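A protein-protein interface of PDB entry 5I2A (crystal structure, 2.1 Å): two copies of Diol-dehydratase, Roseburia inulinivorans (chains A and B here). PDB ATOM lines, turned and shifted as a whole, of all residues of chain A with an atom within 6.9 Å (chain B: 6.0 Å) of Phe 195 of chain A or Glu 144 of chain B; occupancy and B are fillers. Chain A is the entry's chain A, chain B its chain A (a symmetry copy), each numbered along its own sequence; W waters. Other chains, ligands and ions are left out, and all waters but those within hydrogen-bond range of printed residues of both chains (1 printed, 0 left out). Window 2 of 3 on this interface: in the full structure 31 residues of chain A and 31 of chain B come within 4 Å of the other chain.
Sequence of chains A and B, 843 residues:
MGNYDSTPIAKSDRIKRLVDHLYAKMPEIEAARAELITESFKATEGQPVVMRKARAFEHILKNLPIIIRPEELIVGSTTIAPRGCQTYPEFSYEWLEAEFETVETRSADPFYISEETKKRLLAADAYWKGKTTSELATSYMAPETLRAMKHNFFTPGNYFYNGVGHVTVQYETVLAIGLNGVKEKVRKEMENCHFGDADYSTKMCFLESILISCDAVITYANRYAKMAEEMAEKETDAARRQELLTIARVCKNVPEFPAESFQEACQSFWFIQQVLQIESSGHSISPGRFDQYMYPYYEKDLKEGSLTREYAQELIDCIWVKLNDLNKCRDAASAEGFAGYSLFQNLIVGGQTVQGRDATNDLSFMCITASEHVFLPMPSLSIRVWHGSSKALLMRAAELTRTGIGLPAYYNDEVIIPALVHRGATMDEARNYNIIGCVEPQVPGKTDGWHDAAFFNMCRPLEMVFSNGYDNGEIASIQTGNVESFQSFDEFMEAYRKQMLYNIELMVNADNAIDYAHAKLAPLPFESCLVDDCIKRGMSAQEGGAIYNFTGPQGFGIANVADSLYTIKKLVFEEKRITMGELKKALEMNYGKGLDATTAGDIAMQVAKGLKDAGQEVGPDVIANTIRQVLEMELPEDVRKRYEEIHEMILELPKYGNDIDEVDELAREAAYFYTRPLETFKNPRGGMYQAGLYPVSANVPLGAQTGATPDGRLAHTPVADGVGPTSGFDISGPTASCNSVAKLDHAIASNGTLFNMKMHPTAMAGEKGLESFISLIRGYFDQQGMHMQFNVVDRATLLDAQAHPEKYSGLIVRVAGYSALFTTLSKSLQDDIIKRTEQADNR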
ATOM      1  N   CYS A 193      12.146  -5.148 -14.413  1.00  0.00           N
ATOM      2  CA  CYS A 193      12.202  -5.116 -12.948  1.00  0.00           C
ATOM      3  C   CYS A 193      11.311  -4.016 -12.373  1.00  0.00           C
ATOM      4  O   CYS A 193      11.357  -2.874 -12.829  1.00  0.00           O
ATOM      5  CB  CYS A 193      13.643  -4.905 -12.468  1.00  0.00           C
ATOM      6  SG  CYS A 193      14.835  -6.021 -13.224  1.00  0.00           S
ATOM      7  N   HIS A 194      10.502  -4.360 -11.375  1.00  0.00           N
ATOM      8  CA  HIS A 194       9.635  -3.379 -10.723  1.00  0.00           C
ATOM      9  C   HIS A 194      10.033  -3.201  -9.268  1.00  0.00           C
ATOM     10  O   HIS A 194      10.444  -4.157  -8.623  1.00  0.00           O
ATOM     11  CB  HIS A 194       8.168  -3.803 -10.836  1.00  0.00           C
ATOM     12  CG  HIS A 194       7.715  -3.984 -12.249  1.00  0.00           C
ATOM     13  ND1 HIS A 194       7.485  -2.922 -13.096  1.00  0.00           N
ATOM     14  CD2 HIS A 194       7.503  -5.100 -12.979  1.00  0.00           C
ATOM     15  CE1 HIS A 194       7.127  -3.378 -14.282  1.00  0.00           C
ATOM     16  NE2 HIS A 194       7.125  -4.697 -14.236  1.00  0.00           N
ATOM     17  N   PHE A 195       9.910  -1.968  -8.775  1.00  0.00           N
ATOM     18  CA  PHE A 195      10.375  -1.569  -7.445  1.00  0.00           C
ATOM     19  C   PHE A 195      10.052  -2.589  -6.341  1.00  0.00           C
ATOM     20  O   PHE A 195      10.868  -2.821  -5.457  1.00  0.00           O
ATOM     21  CB  PHE A 195       9.772  -0.203  -7.070  1.00  0.00           C
ATOM     22  CG  PHE A 195      10.249   0.944  -7.933  1.00  0.00           C
ATOM     23  CD1 PHE A 195      11.602   1.170  -8.132  1.00  0.00           C
ATOM     24  CD2 PHE A 195       9.336   1.782  -8.559  1.00  0.00           C
ATOM     25  CE1 PHE A 195      12.039   2.224  -8.914  1.00  0.00           C
ATOM     26  CE2 PHE A 195       9.765   2.841  -9.357  1.00  0.00           C
ATOM     27  CZ  PHE A 195      11.119   3.063  -9.532  1.00  0.00           C
ATOM     28  N   GLY A 196       8.873  -3.204  -6.424  1.00  0.00           N
ATOM     29  CA  GLY A 196       8.400  -4.126  -5.405  1.00  0.00           C
ATOM     30  C   GLY A 196       8.786  -5.591  -5.566  1.00  0.00           C
ATOM     31  O   GLY A 196       8.467  -6.392  -4.690  1.00  0.00           O
ATOM     32  N   ASP A 197       9.466  -5.952  -6.660  1.00  0.00           N
ATOM     33  CA  ASP A 197       9.896  -7.343  -6.870  1.00  0.00           C
ATOM     34  C   ASP A 197      10.805  -7.764  -5.711  1.00  0.00           C
ATOM     35  O   ASP A 197      11.637  -6.987  -5.276  1.00  0.00           O
ATOM     36  CB  ASP A 197      10.657  -7.523  -8.202  1.00  0.00           C
ATOM     37  CG  ASP A 197       9.797  -7.223  -9.429  1.00  0.00           C
ATOM     38  OD1 ASP A 197       8.561  -7.177  -9.309  1.00  0.00           O
ATOM     39  OD2 ASP A 197      10.370  -7.009 -10.512  1.00  0.00           O
ATOM     40  N   ALA A 198      10.647  -8.992  -5.232  1.00  0.00           N
ATOM     41  CA  ALA A 198      11.445  -9.486  -4.115  1.00  0.00           C
ATOM     42  C   ALA A 198      12.947  -9.471  -4.412  1.00  0.00           C
ATOM     43  O   ALA A 198      13.753  -9.371  -3.491  1.00  0.00           O
ATOM     44  CB  ALA A 198      10.992 -10.908  -3.714  1.00  0.00           C
ATOM     45  N   TYR A 200      14.407  -7.126  -6.512  1.00  0.00           N
ATOM     46  CA  TYR A 200      14.725  -5.876  -7.203  1.00  0.00           C
ATOM     47  C   TYR A 200      16.060  -5.291  -6.727  1.00  0.00           C
ATOM     48  O   TYR A 200      16.894  -4.923  -7.547  1.00  0.00           O
ATOM     49  CB  TYR A 200      13.610  -4.841  -7.034  1.00  0.00           C
ATOM     50  CG  TYR A 200      13.845  -3.532  -7.806  1.00  0.00           C
ATOM     51  CD1 TYR A 200      14.580  -2.488  -7.248  1.00  0.00           C
ATOM     52  CD2 TYR A 200      13.328  -3.352  -9.088  1.00  0.00           C
ATOM     53  CE1 TYR A 200      14.793  -1.295  -7.949  1.00  0.00           C
ATOM     54  CE2 TYR A 200      13.519  -2.172  -9.787  1.00  0.00           C
ATOM     55  CZ  TYR A 200      14.248  -1.147  -9.215  1.00  0.00           C
ATOM     56  OH  TYR A 200      14.447   0.007  -9.915  1.00  0.00           O
ATOM     57  N   SER A 201      16.275  -5.228  -5.416  1.00  0.00           N
ATOM     58  CA  SER A 201      17.495  -4.602  -4.900  1.00  0.00           C
ATOM     59  C   SER A 201      18.775  -5.253  -5.451  1.00  0.00           C
ATOM     60  O   SER A 201      19.701  -4.566  -5.876  1.00  0.00           O
ATOM     61  CB  SER A 201      17.528  -4.643  -3.371  1.00  0.00           C
ATOM     62  OG  SER A 201      16.591  -3.752  -2.797  1.00  0.00           O
ATOM     63  N   ALA B 142      15.940   2.161  -4.136  1.00  0.00           N
ATOM     64  CA  ALA B 142      15.810   2.944  -5.361  1.00  0.00           C
ATOM     65  C   ALA B 142      15.783   4.450  -5.083  1.00  0.00           C
ATOM     66  O   ALA B 142      15.374   4.875  -4.001  1.00  0.00           O
ATOM     67  CB  ALA B 142      14.570   2.530  -6.118  1.00  0.00           C
ATOM     68  N   PRO B 143      16.256   5.263  -6.050  1.00  0.00           N
ATOM     69  CA  PRO B 143      16.188   6.720  -5.876  1.00  0.00           C
ATOM     70  C   PRO B 143      14.756   7.204  -5.639  1.00  0.00           C
ATOM     71  O   PRO B 143      14.555   8.108  -4.844  1.00  0.00           O
ATOM     72  CB  PRO B 143      16.733   7.264  -7.201  1.00  0.00           C
ATOM     73  CG  PRO B 143      17.586   6.165  -7.746  1.00  0.00           C
ATOM     74  CD  PRO B 143      16.908   4.887  -7.316  1.00  0.00           C
ATOM     75  N   GLU B 144      13.786   6.599  -6.317  1.00  0.00           N
ATOM     76  CA  GLU B 144      12.390   6.986  -6.152  1.00  0.00           C
ATOM     77  C   GLU B 144      11.914   6.690  -4.722  1.00  0.00           C
ATOM     78  O   GLU B 144      11.118   7.428  -4.161  1.00  0.00           O
ATOM     79  CB  GLU B 144      11.498   6.274  -7.181  1.00  0.00           C
ATOM     80  CG  GLU B 144      11.690   6.758  -8.632  1.00  0.00           C
ATOM     81  CD  GLU B 144      12.895   6.136  -9.341  1.00  0.00           C
ATOM     82  OE1 GLU B 144      13.725   5.467  -8.696  1.00  0.00           O
ATOM     83  OE2 GLU B 144      13.003   6.306 -10.565  1.00  0.00           O
ATOM     84  N   THR B 145      12.422   5.604  -4.152  1.00  0.00           N
ATOM     85  CA  THR B 145      12.148   5.244  -2.770  1.00  0.00           C
ATOM     86  C   THR B 145      12.697   6.281  -1.791  1.00  0.00           C
ATOM     87  O   THR B 145      12.010   6.677  -0.841  1.00  0.00           O
ATOM     88  CB  THR B 145      12.743   3.863  -2.444  1.00  0.00           C
ATOM     89  OG1 THR B 145      12.200   2.895  -3.349  1.00  0.00           O
ATOM     90  CG2 THR B 145      12.433   3.462  -1.013  1.00  0.00           C
ATOM     91  N   LEU B 146      13.934   6.717  -2.017  1.00  0.00           N
ATOM     92  CA  LEU B 146      14.524   7.742  -1.170  1.00  0.00           C
ATOM     93  C   LEU B 146      13.699   9.031  -1.254  1.00  0.00           C
ATOM     94  O   LEU B 146      13.518   9.721  -0.256  1.00  0.00           O
ATOM     95  CB  LEU B 146      15.988   7.998  -1.556  1.00  0.00           C
ATOM     96  CG  LEU B 146      16.940   6.801  -1.387  1.00  0.00           C
ATOM     97  CD1 LEU B 146      18.346   7.112  -1.926  1.00  0.00           C
ATOM     98  CD2 LEU B 146      17.009   6.384   0.068  1.00  0.00           C
ATOM     99  N   ARG B 147      13.197   9.337  -2.448  1.00  0.00           N
ATOM    100  CA  ARG B 147      12.393  10.536  -2.655  1.00  0.00           C
ATOM    101  C   ARG B 147      11.087  10.444  -1.868  1.00  0.00           C
ATOM    102  O   ARG B 147      10.682  11.400  -1.212  1.00  0.00           O
ATOM    103  CB  ARG B 147      12.098  10.761  -4.145  1.00  0.00           C
ATOM    104  CG  ARG B 147      11.288  12.024  -4.421  1.00  0.00           C
ATOM    105  CD  ARG B 147      11.055  12.242  -5.916  1.00  0.00           C
ATOM    106  NE  ARG B 147      10.239  11.170  -6.466  1.00  0.00           N
ATOM    107  CZ  ARG B 147      10.042  10.946  -7.762  1.00  0.00           C
ATOM    108  NH1 ARG B 147      10.605  11.728  -8.674  1.00  0.00           N
ATOM    109  NH2 ARG B 147       9.287   9.928  -8.148  1.00  0.00           N
ATOM    110  N   ALA B 148      10.441   9.287  -1.927  1.00  0.00           N
ATOM    111  CA  ALA B 148       9.186   9.088  -1.206  1.00  0.00           C
ATOM    112  C   ALA B 148       9.378   9.297   0.302  1.00  0.00           C
ATOM    113  O   ALA B 148       8.530   9.882   0.977  1.00  0.00           O
ATOM    114  CB  ALA B 148       8.628   7.698  -1.497  1.00  0.00           C
ATOM    115  N   MET B 149      10.511   8.846   0.820  1.00  0.00           N
ATOM    116  CA  MET B 149      10.772   8.961   2.248  1.00  0.00           C
ATOM    117  C   MET B 149      11.079  10.402   2.613  1.00  0.00           C
ATOM    118  O   MET B 149      10.664  10.882   3.661  1.00  0.00           O
ATOM    119  CB  MET B 149      11.916   8.038   2.659  1.00  0.00           C
ATOM    120  CG  MET B 149      11.535   6.552   2.569  1.00  0.00           C
ATOM    121  SD  MET B 149      12.926   5.466   2.935  1.00  0.00           S
ATOM    122  CE  MET B 149      13.934   5.674   1.526  1.00  0.00           C
ATOM    123  N   TYR B 502       1.384   3.479  -6.186  1.00  0.00           N
ATOM    124  CA  TYR B 502       2.756   3.885  -6.483  1.00  0.00           C
ATOM    125  C   TYR B 502       3.623   3.937  -5.225  1.00  0.00           C
ATOM    126  O   TYR B 502       4.726   3.384  -5.189  1.00  0.00           O
ATOM    127  CB  TYR B 502       2.774   5.247  -7.169  1.00  0.00           C
ATOM    128  CG  TYR B 502       4.166   5.731  -7.529  1.00  0.00           C
ATOM    129  CD1 TYR B 502       4.853   5.179  -8.602  1.00  0.00           C
ATOM    130  CD2 TYR B 502       4.789   6.731  -6.796  1.00  0.00           C
ATOM    131  CE1 TYR B 502       6.115   5.622  -8.937  1.00  0.00           C
ATOM    132  CE2 TYR B 502       6.057   7.179  -7.124  1.00  0.00           C
ATOM    133  CZ  TYR B 502       6.714   6.620  -8.195  1.00  0.00           C
ATOM    134  OH  TYR B 502       7.969   7.063  -8.536  1.00  0.00           O
ATOM    135  N   GLU B 505       4.304   0.552  -3.348  1.00  0.00           N
ATOM    136  CA  GLU B 505       5.337  -0.274  -3.957  1.00  0.00           C
ATOM    137  C   GLU B 505       6.745   0.224  -3.591  1.00  0.00           C
ATOM    138  O   GLU B 505       7.675  -0.574  -3.417  1.00  0.00           O
ATOM    139  CB  GLU B 505       5.167  -0.328  -5.479  1.00  0.00           C
ATOM    140  CG  GLU B 505       6.211  -1.227  -6.139  1.00  0.00           C
ATOM    141  CD  GLU B 505       5.860  -1.632  -7.574  1.00  0.00           C
ATOM    142  OE1 GLU B 505       4.919  -1.051  -8.152  1.00  0.00           O
ATOM    143  OE2 GLU B 505       6.527  -2.546  -8.104  1.00  0.00           O
ATOM    144  N   LEU B 506       6.901   1.538  -3.472  1.00  0.00           N
ATOM    145  CA  LEU B 506       8.159   2.103  -2.992  1.00  0.00           C
ATOM    146  C   LEU B 506       8.463   1.697  -1.541  1.00  0.00           C
ATOM    147  O   LEU B 506       9.621   1.493  -1.174  1.00  0.00           O
ATOM    148  CB  LEU B 506       8.133   3.628  -3.119  1.00  0.00           C
ATOM    149  CG  LEU B 506       8.058   4.147  -4.558  1.00  0.00           C
ATOM    150  CD1 LEU B 506       8.138   5.664  -4.602  1.00  0.00           C
ATOM    151  CD2 LEU B 506       9.178   3.526  -5.391  1.00  0.00           C
ATOM    152  N   VAL B 508       7.525  -1.111  -0.243  1.00  0.00           N
ATOM    153  CA  VAL B 508       7.958  -2.502  -0.398  1.00  0.00           C
ATOM    154  C   VAL B 508       9.450  -2.516  -0.785  1.00  0.00           C
ATOM    155  O   VAL B 508      10.238  -3.281  -0.238  1.00  0.00           O
ATOM    156  CB  VAL B 508       7.093  -3.260  -1.438  1.00  0.00           C
ATOM    157  CG1 VAL B 508       7.667  -4.662  -1.733  1.00  0.00           C
ATOM    158  CG2 VAL B 508       5.624  -3.363  -0.964  1.00  0.00           C
ATOM    159  N   ASN B 509       9.839  -1.625  -1.684  1.00  0.00           N
ATOM    160  CA  ASN B 509      11.250  -1.505  -2.050  1.00  0.00           C
ATOM    161  C   ASN B 509      12.135  -1.196  -0.830  1.00  0.00           C
ATOM    162  O   ASN B 509      13.171  -1.822  -0.641  1.00  0.00           O
ATOM    163  CB  ASN B 509      11.433  -0.427  -3.133  1.00  0.00           C
ATOM    164  CG  ASN B 509      12.874  -0.314  -3.618  1.00  0.00           C
ATOM    165  OD1 ASN B 509      13.622   0.531  -3.146  1.00  0.00           O
ATOM    166  ND2 ASN B 509      13.263  -1.170  -4.570  1.00  0.00           N
ATOM    167  N   ASN B 512      12.225  -4.296   1.610  1.00  0.00           N
ATOM    168  CA  ASN B 512      12.981  -5.381   0.987  1.00  0.00           C
ATOM    169  C   ASN B 512      14.482  -5.058   0.983  1.00  0.00           C
ATOM    170  O   ASN B 512      15.308  -5.933   1.199  1.00  0.00           O
ATOM    171  CB  ASN B 512      12.476  -5.664  -0.440  1.00  0.00           C
ATOM    172  CG  ASN B 512      11.132  -6.408  -0.450  1.00  0.00           C
ATOM    173  OD1 ASN B 512      10.640  -6.832   0.595  1.00  0.00           O
ATOM    174  ND2 ASN B 512      10.560  -6.590  -1.633  1.00  0.00           N
HETATM  175  O   HOH W   1      11.609  -4.838  -3.745  1.00  0.00           O
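Water W1 lies within hydrogen-bond range of O of Asp 197 of chain A (2.6 Å), O of Phe 195 of chain A (2.7 Å) and ND2 of Asn 512 of chain B (2.9 Å).
Of chain B, only Ala 142 (3.8 Å), Glu 144 (3.6 Å), Glu 505 (3.5 Å), Leu 506 (3.6 Å) and Asn 509 (3.0 Å) come within 4 Å of Phe 195 of chain A.
Of the printed residues of chain B, Asp 197 of chain A touches Asn 512 (3.8 Å).
Of the printed residues of chain B, Tyr 200 of chain A touches Asn 509.
Printed residues of chain A within 4 Å of Ala 142 of chain B: Phe 195 (3.8 Å).
Glu 144 of chain B touches one residue of chain A.
Of the printed residues of chain A, Leu 506 of chain B touches Phe 195 (3.6 Å).
The nearest residue of chain B that does not touch Phe 195 of chain A is Tyr 502 of chain B (4.6 Å).
Of the 8 printed residues of chain A, 6 touch a printed residue of chain B.
Hydrophobic or aromatic side chains of chain A within 4 Å of the printed part of chain B: His 194, Phe 195 and Tyr 200.
Along chain A the printed residues that touch a printed residue of chain B span positions 194 to 200.
Among the printed residues, 12 pairs touch across the chains.
Among the printed residues, no Asp or Glu carboxylate lies within 4 Å of a Lys or Arg side-chain nitrogen of the other chain.
No position is printed for both chains.
Of the 12 pairs that touch across the chains among the printed residues, none has its exchanged pair printed and touching as well.
The backbone NH of His 194 of chain A is in hydrogen-bond range of the side-chain carboxylate of Asp 197 of chain A (2.8 Å).
OD1 of Asn 509 of chain B lies within hydrogen-bond range of N of Ala 142 of chain B, 3.0 Å away.
The side-chain hydroxyl (OG1) of Thr 145 of chain B sits at hydrogen-bond distance from the side-chain amide oxygen (OD1) of Asn 509 of chain B, 2.8 Å away.
OE2 of Glu 505 of chain B sits at hydrogen-bond distance from N of Phe 195 of chain A.
O of Phe 195 of chain A is in hydrogen-bond range of ND2 of Asn 509 of chain B (3.0 Å).
OE2 of Glu 505 of chain B sits at hydrogen-bond distance from N of Gly 196 of chain A, at 3.0 Å.
Among the printed residues, pairs that only touch across the chains: Tyr 200 of chain A with Asn 509 of chain B (3.3 Å), His 194 of chain A with Glu 505 of chain B (3.4 Å), Gly 196 of chain A with Val 508 of chain B (3.5 Å), Phe 195 of chain A with Glu 144 of chain B (3.6 Å), Phe 195 of chain A with Leu 506 of chain B (3.6 Å), Gly 196 of chain A with Asn 512 of chain B (3.7 Å), Phe 195 of chain A with Ala 142 of chain B (3.8 Å), Asp 197 of chain A with Asn 512 of chain B (3.8 Å) and Ala 198 of chain A with Asn 512 of chain B (3.9 Å).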
